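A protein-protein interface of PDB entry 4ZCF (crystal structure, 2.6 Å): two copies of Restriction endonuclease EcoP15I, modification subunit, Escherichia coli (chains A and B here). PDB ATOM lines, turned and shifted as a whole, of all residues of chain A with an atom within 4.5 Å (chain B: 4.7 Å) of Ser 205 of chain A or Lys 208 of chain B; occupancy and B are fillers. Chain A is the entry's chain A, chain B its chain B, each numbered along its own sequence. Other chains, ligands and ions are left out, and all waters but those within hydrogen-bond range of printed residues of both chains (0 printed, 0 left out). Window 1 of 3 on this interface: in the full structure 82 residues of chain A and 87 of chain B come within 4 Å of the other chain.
Of the 7 printed residues of chain A, 5 touch a printed residue of chain B.
Printed residues of chain A that touch a printed residue of chain B: Phe 204, Ser 205, Gln 206, Lys 208 and Leu 209.
Hydrophobic or aromatic side chains of chain A that line the printed part of chain B: Phe 204 and Leu 209.
Along chain A the printed residues that touch a printed residue of chain B span positions 204 to 209.
Among the printed residues, no Asp or Glu carboxylate lies within 4 Å of a Lys or Arg side-chain nitrogen of the other chain.
Ser 205 of chain B touches its own counterpart, Ser 205 of chain A.
Ser 205 of chain A touches Lys 208 of chain B, and with the chains exchanged Lys 208 of chain A touches Ser 205 of chain B.
Ser 205 of chain A touches Leu 209 of chain B, and with the chains exchanged Leu 209 of chain A touches Ser 205 of chain B.
Gln 206 of chain A touches Leu 209 of chain B, and with the chains exchanged Leu 209 of chain A touches Gln 206 of chain B.
Of the 9 pairs that touch across the chains among the printed residues, 9 have their exchanged pair printed and touching as well.
Among the printed residues, merely in contact across the chains: Ser 205 of chain A with Lys 208 of chain B (3.1 Å), Gln 206 of chain A with Leu 209 of chain B (3.1 Å), Phe 204 of chain A with Phe 204 of chain B (3.3 Å), Leu 209 of chain A with Gln 206 of chain B (3.3 Å), Lys 208 of chain A with Ser 205 of chain B (3.5 Å), Leu 209 of chain A with Leu 209 of chain B (3.6 Å), Ser 205 of chain A with Ser 205 of chain B (3.7 Å), Ser 205 of chain A with Leu 209 of chain B (3.9 Å) and Leu 209 of chain A with Ser 205 of chain B (3.9 Å).
The side-chain amino group (NZ) of Lys 208 of chain B lies within salt-bridge range of the side-chain carboxylate (OE2) of Glu 217 of chain B.
The side-chain carboxylate (OD2) of Asp 212 of chain B lies within salt-bridge range of the side-chain amino group (NZ) of Lys 208 of chain B.
The backbone carbonyl oxygen of Lys 208 of chain B sits close to the side-chain hydroxyl of Tyr 247 of chain B (3.3 Å).
Ser 205 of chain A touches just these residues of chain B: Ser 205, Lys 208 and Leu 209.
Leu 207 of chain A touches none of the printed residues of chain B.
Of the printed residues of chain A, Phe 204 of chain B touches Phe 204 (3.3 Å).
Printed residues of chain A within 4 Å of Ser 205 of chain B: Ser 205, Lys 208 and Leu 209.
Lys 208 of chain B touches just one residue of chain A: Ser 205 (3.1 Å).
Tyr 247 of chain B touches none of the printed residues of chain A.
The nearest printed residue of chain A that does not touch Lys 208 of chain B is Gln 206 of chain A (4.9 Å).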
ATOM      1  N   GLU A 203      21.051  16.945  16.888  1.00  0.00           N
ATOM      2  CA  GLU A 203      21.916  15.804  17.222  1.00  0.00           C
ATOM      3  C   GLU A 203      21.360  14.830  18.264  1.00  0.00           C
ATOM      4  O   GLU A 203      22.101  13.948  18.706  1.00  0.00           O
ATOM      5  CB  GLU A 203      23.318  16.301  17.660  1.00  0.00           C
ATOM      6  CG  GLU A 203      24.033  17.164  16.634  1.00  0.00           C
ATOM      7  CD  GLU A 203      24.394  16.468  15.334  1.00  0.00           C
ATOM      8  OE1 GLU A 203      24.569  15.229  15.354  1.00  0.00           O
ATOM      9  OE2 GLU A 203      24.500  17.161  14.295  1.00  0.00           O
ATOM     10  N   PHE A 204      20.078  14.968  18.648  1.00  0.00           N
ATOM     11  CA  PHE A 204      19.452  14.101  19.657  1.00  0.00           C
ATOM     12  C   PHE A 204      19.669  12.602  19.405  1.00  0.00           C
ATOM     13  O   PHE A 204      20.259  11.944  20.256  1.00  0.00           O
ATOM     14  CB  PHE A 204      17.963  14.462  19.890  1.00  0.00           C
ATOM     15  CG  PHE A 204      17.168  13.554  20.810  1.00  0.00           C
ATOM     16  CD1 PHE A 204      17.687  13.141  22.034  1.00  0.00           C
ATOM     17  CD2 PHE A 204      15.875  13.169  20.483  1.00  0.00           C
ATOM     18  CE1 PHE A 204      16.942  12.329  22.894  1.00  0.00           C
ATOM     19  CE2 PHE A 204      15.135  12.342  21.346  1.00  0.00           C
ATOM     20  CZ  PHE A 204      15.676  11.930  22.542  1.00  0.00           C
ATOM     21  N   SER A 205      19.244  12.085  18.233  1.00  0.00           N
ATOM     22  CA  SER A 205      19.366  10.664  17.847  1.00  0.00           C
ATOM     23  C   SER A 205      20.809  10.199  17.748  1.00  0.00           C
ATOM     24  O   SER A 205      21.140   9.162  18.325  1.00  0.00           O
ATOM     25  CB  SER A 205      18.624  10.394  16.543  1.00  0.00           C
ATOM     26  OG  SER A 205      17.473  11.218  16.450  1.00  0.00           O
ATOM     27  N   GLN A 206      21.679  10.998  17.089  1.00  0.00           N
ATOM     28  CA  GLN A 206      23.128  10.734  16.919  1.00  0.00           C
ATOM     29  C   GLN A 206      23.887  10.668  18.230  1.00  0.00           C
ATOM     30  O   GLN A 206      24.761   9.813  18.370  1.00  0.00           O
ATOM     31  CB  GLN A 206      23.778  11.767  16.002  1.00  0.00           C
ATOM     32  CG  GLN A 206      23.398  11.595  14.525  1.00  0.00           C
ATOM     33  CD  GLN A 206      22.031  12.130  14.126  1.00  0.00           C
ATOM     34  OE1 GLN A 206      21.287  12.782  14.893  1.00  0.00           O
ATOM     35  NE2 GLN A 206      21.691  11.875  12.886  1.00  0.00           N
ATOM     36  N   LEU A 207      23.557  11.545  19.202  1.00  0.00           N
ATOM     37  CA  LEU A 207      24.188  11.533  20.527  1.00  0.00           C
ATOM     38  C   LEU A 207      23.703  10.350  21.325  1.00  0.00           C
ATOM     39  O   LEU A 207      24.499   9.701  21.996  1.00  0.00           O
ATOM     40  CB  LEU A 207      23.849  12.820  21.278  1.00  0.00           C
ATOM     41  CG  LEU A 207      24.194  12.906  22.772  1.00  0.00           C
ATOM     42  CD1 LEU A 207      25.748  12.912  23.031  1.00  0.00           C
ATOM     43  CD2 LEU A 207      23.476  14.083  23.389  1.00  0.00           C
ATOM     44  N   LYS A 208      22.401  10.090  21.283  1.00  0.00           N
ATOM     45  CA  LYS A 208      21.756   9.001  21.993  1.00  0.00           C
ATOM     46  C   LYS A 208      22.347   7.685  21.540  1.00  0.00           C
ATOM     47  O   LYS A 208      22.619   6.827  22.388  1.00  0.00           O
ATOM     48  CB  LYS A 208      20.228   9.022  21.769  1.00  0.00           C
ATOM     49  CG  LYS A 208      19.440   9.695  22.880  1.00  0.00           C
ATOM     50  CD  LYS A 208      19.395   8.871  24.196  1.00  0.00           C
ATOM     51  CE  LYS A 208      18.364   7.768  24.213  1.00  0.00           C
ATOM     52  NZ  LYS A 208      18.855   6.538  23.531  1.00  0.00           N
ATOM     53  N   LEU A 209      22.597   7.550  20.213  1.00  0.00           N
ATOM     54  CA  LEU A 209      23.242   6.363  19.638  1.00  0.00           C
ATOM     55  C   LEU A 209      24.722   6.224  20.020  1.00  0.00           C
ATOM     56  O   LEU A 209      25.150   5.103  20.320  1.00  0.00           O
ATOM     57  CB  LEU A 209      22.989   6.207  18.120  1.00  0.00           C
ATOM     58  CG  LEU A 209      21.513   5.887  17.706  1.00  0.00           C
ATOM     59  CD1 LEU A 209      21.428   5.514  16.261  1.00  0.00           C
ATOM     60  CD2 LEU A 209      20.921   4.750  18.522  1.00  0.00           C
ATOM     61  N   PHE B 204      12.894   5.608  19.030  1.00  0.00           N
ATOM     62  CA  PHE B 204      12.905   6.999  18.556  1.00  0.00           C
ATOM     63  C   PHE B 204      14.133   7.359  17.731  1.00  0.00           C
ATOM     64  O   PHE B 204      13.979   8.011  16.690  1.00  0.00           O
ATOM     65  CB  PHE B 204      12.747   8.002  19.705  1.00  0.00           C
ATOM     66  CG  PHE B 204      12.605   9.435  19.232  1.00  0.00           C
ATOM     67  CD1 PHE B 204      13.724  10.230  19.016  1.00  0.00           C
ATOM     68  CD2 PHE B 204      11.364   9.960  18.920  1.00  0.00           C
ATOM     69  CE1 PHE B 204      13.592  11.529  18.518  1.00  0.00           C
ATOM     70  CE2 PHE B 204      11.234  11.279  18.482  1.00  0.00           C
ATOM     71  CZ  PHE B 204      12.343  12.057  18.295  1.00  0.00           C
ATOM     72  N   SER B 205      15.359   6.997  18.214  1.00  0.00           N
ATOM     73  CA  SER B 205      16.585   7.352  17.492  1.00  0.00           C
ATOM     74  C   SER B 205      16.664   6.615  16.167  1.00  0.00           C
ATOM     75  O   SER B 205      16.861   7.243  15.132  1.00  0.00           O
ATOM     76  CB  SER B 205      17.826   7.135  18.342  1.00  0.00           C
ATOM     77  OG  SER B 205      17.710   7.842  19.564  1.00  0.00           O
ATOM     78  N   GLN B 206      16.399   5.307  16.205  1.00  0.00           N
ATOM     79  CA  GLN B 206      16.386   4.391  15.068  1.00  0.00           C
ATOM     80  C   GLN B 206      15.330   4.812  14.056  1.00  0.00           C
ATOM     81  O   GLN B 206      15.660   4.909  12.865  1.00  0.00           O
ATOM     82  CB  GLN B 206      16.218   2.929  15.538  1.00  0.00           C
ATOM     83  CG  GLN B 206      17.357   2.448  16.452  1.00  0.00           C
ATOM     84  CD  GLN B 206      17.303   2.970  17.890  1.00  0.00           C
ATOM     85  OE1 GLN B 206      16.353   3.623  18.347  1.00  0.00           O
ATOM     86  NE2 GLN B 206      18.318   2.667  18.650  1.00  0.00           N
ATOM     87  N   LEU B 207      14.106   5.179  14.531  1.00  0.00           N
ATOM     88  CA  LEU B 207      13.045   5.701  13.653  1.00  0.00           C
ATOM     89  C   LEU B 207      13.502   6.971  12.919  1.00  0.00           C
ATOM     90  O   LEU B 207      13.427   7.023  11.709  1.00  0.00           O
ATOM     91  CB  LEU B 207      11.721   5.970  14.413  1.00  0.00           C
ATOM     92  CG  LEU B 207      10.535   6.447  13.538  1.00  0.00           C
ATOM     93  CD1 LEU B 207      10.144   5.406  12.467  1.00  0.00           C
ATOM     94  CD2 LEU B 207       9.341   6.878  14.381  1.00  0.00           C
ATOM     95  N   LYS B 208      14.002   7.966  13.644  1.00  0.00           N
ATOM     96  CA  LYS B 208      14.493   9.223  13.107  1.00  0.00           C
ATOM     97  C   LYS B 208      15.503   9.006  11.998  1.00  0.00           C
ATOM     98  O   LYS B 208      15.338   9.540  10.901  1.00  0.00           O
ATOM     99  CB  LYS B 208      15.080  10.085  14.242  1.00  0.00           C
ATOM    100  CG  LYS B 208      15.897  11.306  13.798  1.00  0.00           C
ATOM    101  CD  LYS B 208      15.059  12.484  13.280  1.00  0.00           C
ATOM    102  CE  LYS B 208      15.898  13.701  12.944  1.00  0.00           C
ATOM    103  NZ  LYS B 208      17.070  13.373  12.070  1.00  0.00           N
ATOM    104  N   LEU B 209      16.506   8.188  12.265  1.00  0.00           N
ATOM    105  CA  LEU B 209      17.572   7.911  11.308  1.00  0.00           C
ATOM    106  C   LEU B 209      17.118   7.146  10.046  1.00  0.00           C
ATOM    107  O   LEU B 209      17.579   7.479   8.950  1.00  0.00           O
ATOM    108  CB  LEU B 209      18.840   7.326  12.000  1.00  0.00           C
ATOM    109  CG  LEU B 209      19.460   8.174  13.164  1.00  0.00           C
ATOM    110  CD1 LEU B 209      20.857   7.760  13.443  1.00  0.00           C
ATOM    111  CD2 LEU B 209      19.522   9.640  12.841  1.00  0.00           C
ATOM    112  N   VAL B 210      16.167   6.191  10.187  1.00  0.00           N
ATOM    113  CA  VAL B 210      15.613   5.461   9.045  1.00  0.00           C
ATOM    114  C   VAL B 210      14.695   6.374   8.190  1.00  0.00           C
ATOM    115  O   VAL B 210      14.641   6.225   6.966  1.00  0.00           O
ATOM    116  CB  VAL B 210      15.016   4.069   9.419  1.00  0.00           C
ATOM    117  CG1 VAL B 210      13.669   4.178  10.149  1.00  0.00           C
ATOM    118  CG2 VAL B 210      14.921   3.146   8.211  1.00  0.00           C
ATOM    119  N   CYS B 211      14.019   7.358   8.822  1.00  0.00           N
ATOM    120  CA  CYS B 211      13.221   8.340   8.077  1.00  0.00           C
ATOM    121  C   CYS B 211      14.132   9.261   7.261  1.00  0.00           C
ATOM    122  O   CYS B 211      13.779   9.599   6.137  1.00  0.00           O
ATOM    123  CB  CYS B 211      12.311   9.121   9.002  1.00  0.00           C
ATOM    124  SG  CYS B 211      10.934   8.156   9.649  1.00  0.00           S
ATOM    125  N   ASP B 212      15.319   9.625   7.801  1.00  0.00           N
ATOM    126  CA  ASP B 212      16.336  10.392   7.060  1.00  0.00           C
ATOM    127  C   ASP B 212      16.809   9.585   5.839  1.00  0.00           C
ATOM    128  O   ASP B 212      16.892  10.138   4.744  1.00  0.00           O
ATOM    129  CB  ASP B 212      17.552  10.761   7.932  1.00  0.00           C
ATOM    130  CG  ASP B 212      17.266  11.733   9.055  1.00  0.00           C
ATOM    131  OD1 ASP B 212      16.289  12.515   8.934  1.00  0.00           O
ATOM    132  OD2 ASP B 212      18.017  11.716  10.060  1.00  0.00           O
ATOM    133  N   GLU B 217      16.963  14.132   5.525  1.00  0.00           N
ATOM    134  CA  GLU B 217      16.893  15.021   6.694  1.00  0.00           C
ATOM    135  C   GLU B 217      16.298  16.406   6.472  1.00  0.00           C
ATOM    136  O   GLU B 217      15.660  16.941   7.368  1.00  0.00           O
ATOM    137  CB  GLU B 217      18.213  15.078   7.472  1.00  0.00           C
ATOM    138  CG  GLU B 217      17.995  15.410   8.951  1.00  0.00           C
ATOM    139  CD  GLU B 217      19.211  15.368   9.853  1.00  0.00           C
ATOM    140  OE1 GLU B 217      20.346  15.416   9.331  1.00  0.00           O
ATOM    141  OE2 GLU B 217      19.026  15.280  11.089  1.00  0.00           O
ATOM    142  N   HIS B 220      12.469  16.740   7.138  1.00  0.00           N
ATOM    143  CA  HIS B 220      12.058  16.572   8.524  1.00  0.00           C
ATOM    144  C   HIS B 220      11.283  17.814   8.916  1.00  0.00           C
ATOM    145  O   HIS B 220      11.837  18.908   8.883  1.00  0.00           O
ATOM    146  CB  HIS B 220      13.315  16.383   9.423  1.00  0.00           C
ATOM    147  CG  HIS B 220      13.026  16.239  10.889  1.00  0.00           C
ATOM    148  ND1 HIS B 220      13.551  17.124  11.815  1.00  0.00           N
ATOM    149  CD2 HIS B 220      12.251  15.340  11.537  1.00  0.00           C
ATOM    150  CE1 HIS B 220      13.087  16.732  12.993  1.00  0.00           C
ATOM    151  NE2 HIS B 220      12.316  15.651  12.875  1.00  0.00           N
ATOM    152  N   ILE B 245       7.174  11.623  15.353  1.00  0.00           N
ATOM    153  CA  ILE B 245       8.141  12.044  14.346  1.00  0.00           C
ATOM    154  C   ILE B 245       7.323  12.441  13.111  1.00  0.00           C
ATOM    155  O   ILE B 245       6.497  11.648  12.665  1.00  0.00           O
ATOM    156  CB  ILE B 245       9.181  10.907  14.090  1.00  0.00           C
ATOM    157  CG1 ILE B 245      10.167  10.830  15.265  1.00  0.00           C
ATOM    158  CG2 ILE B 245       9.921  11.088  12.768  1.00  0.00           C
ATOM    159  CD1 ILE B 245      11.317   9.760  15.197  1.00  0.00           C
ATOM    160  N   TYR B 247       7.526  13.991   9.114  1.00  0.00           N
ATOM    161  CA  TYR B 247       8.304  14.221   7.892  1.00  0.00           C
ATOM    162  C   TYR B 247       7.398  14.663   6.758  1.00  0.00           C
ATOM    163  O   TYR B 247       6.175  14.541   6.838  1.00  0.00           O
ATOM    164  CB  TYR B 247       9.090  12.959   7.466  1.00  0.00           C
ATOM    165  CG  TYR B 247      10.421  12.832   8.167  1.00  0.00           C
ATOM    166  CD1 TYR B 247      10.491  12.438   9.498  1.00  0.00           C
ATOM    167  CD2 TYR B 247      11.614  13.082   7.497  1.00  0.00           C
ATOM    168  CE1 TYR B 247      11.711  12.335  10.159  1.00  0.00           C
ATOM    169  CE2 TYR B 247      12.840  12.981   8.150  1.00  0.00           C
ATOM    170  CZ  TYR B 247      12.879  12.617   9.487  1.00  0.00           C
ATOM    171  OH  TYR B 247      14.055  12.480  10.180  1.00  0.00           O
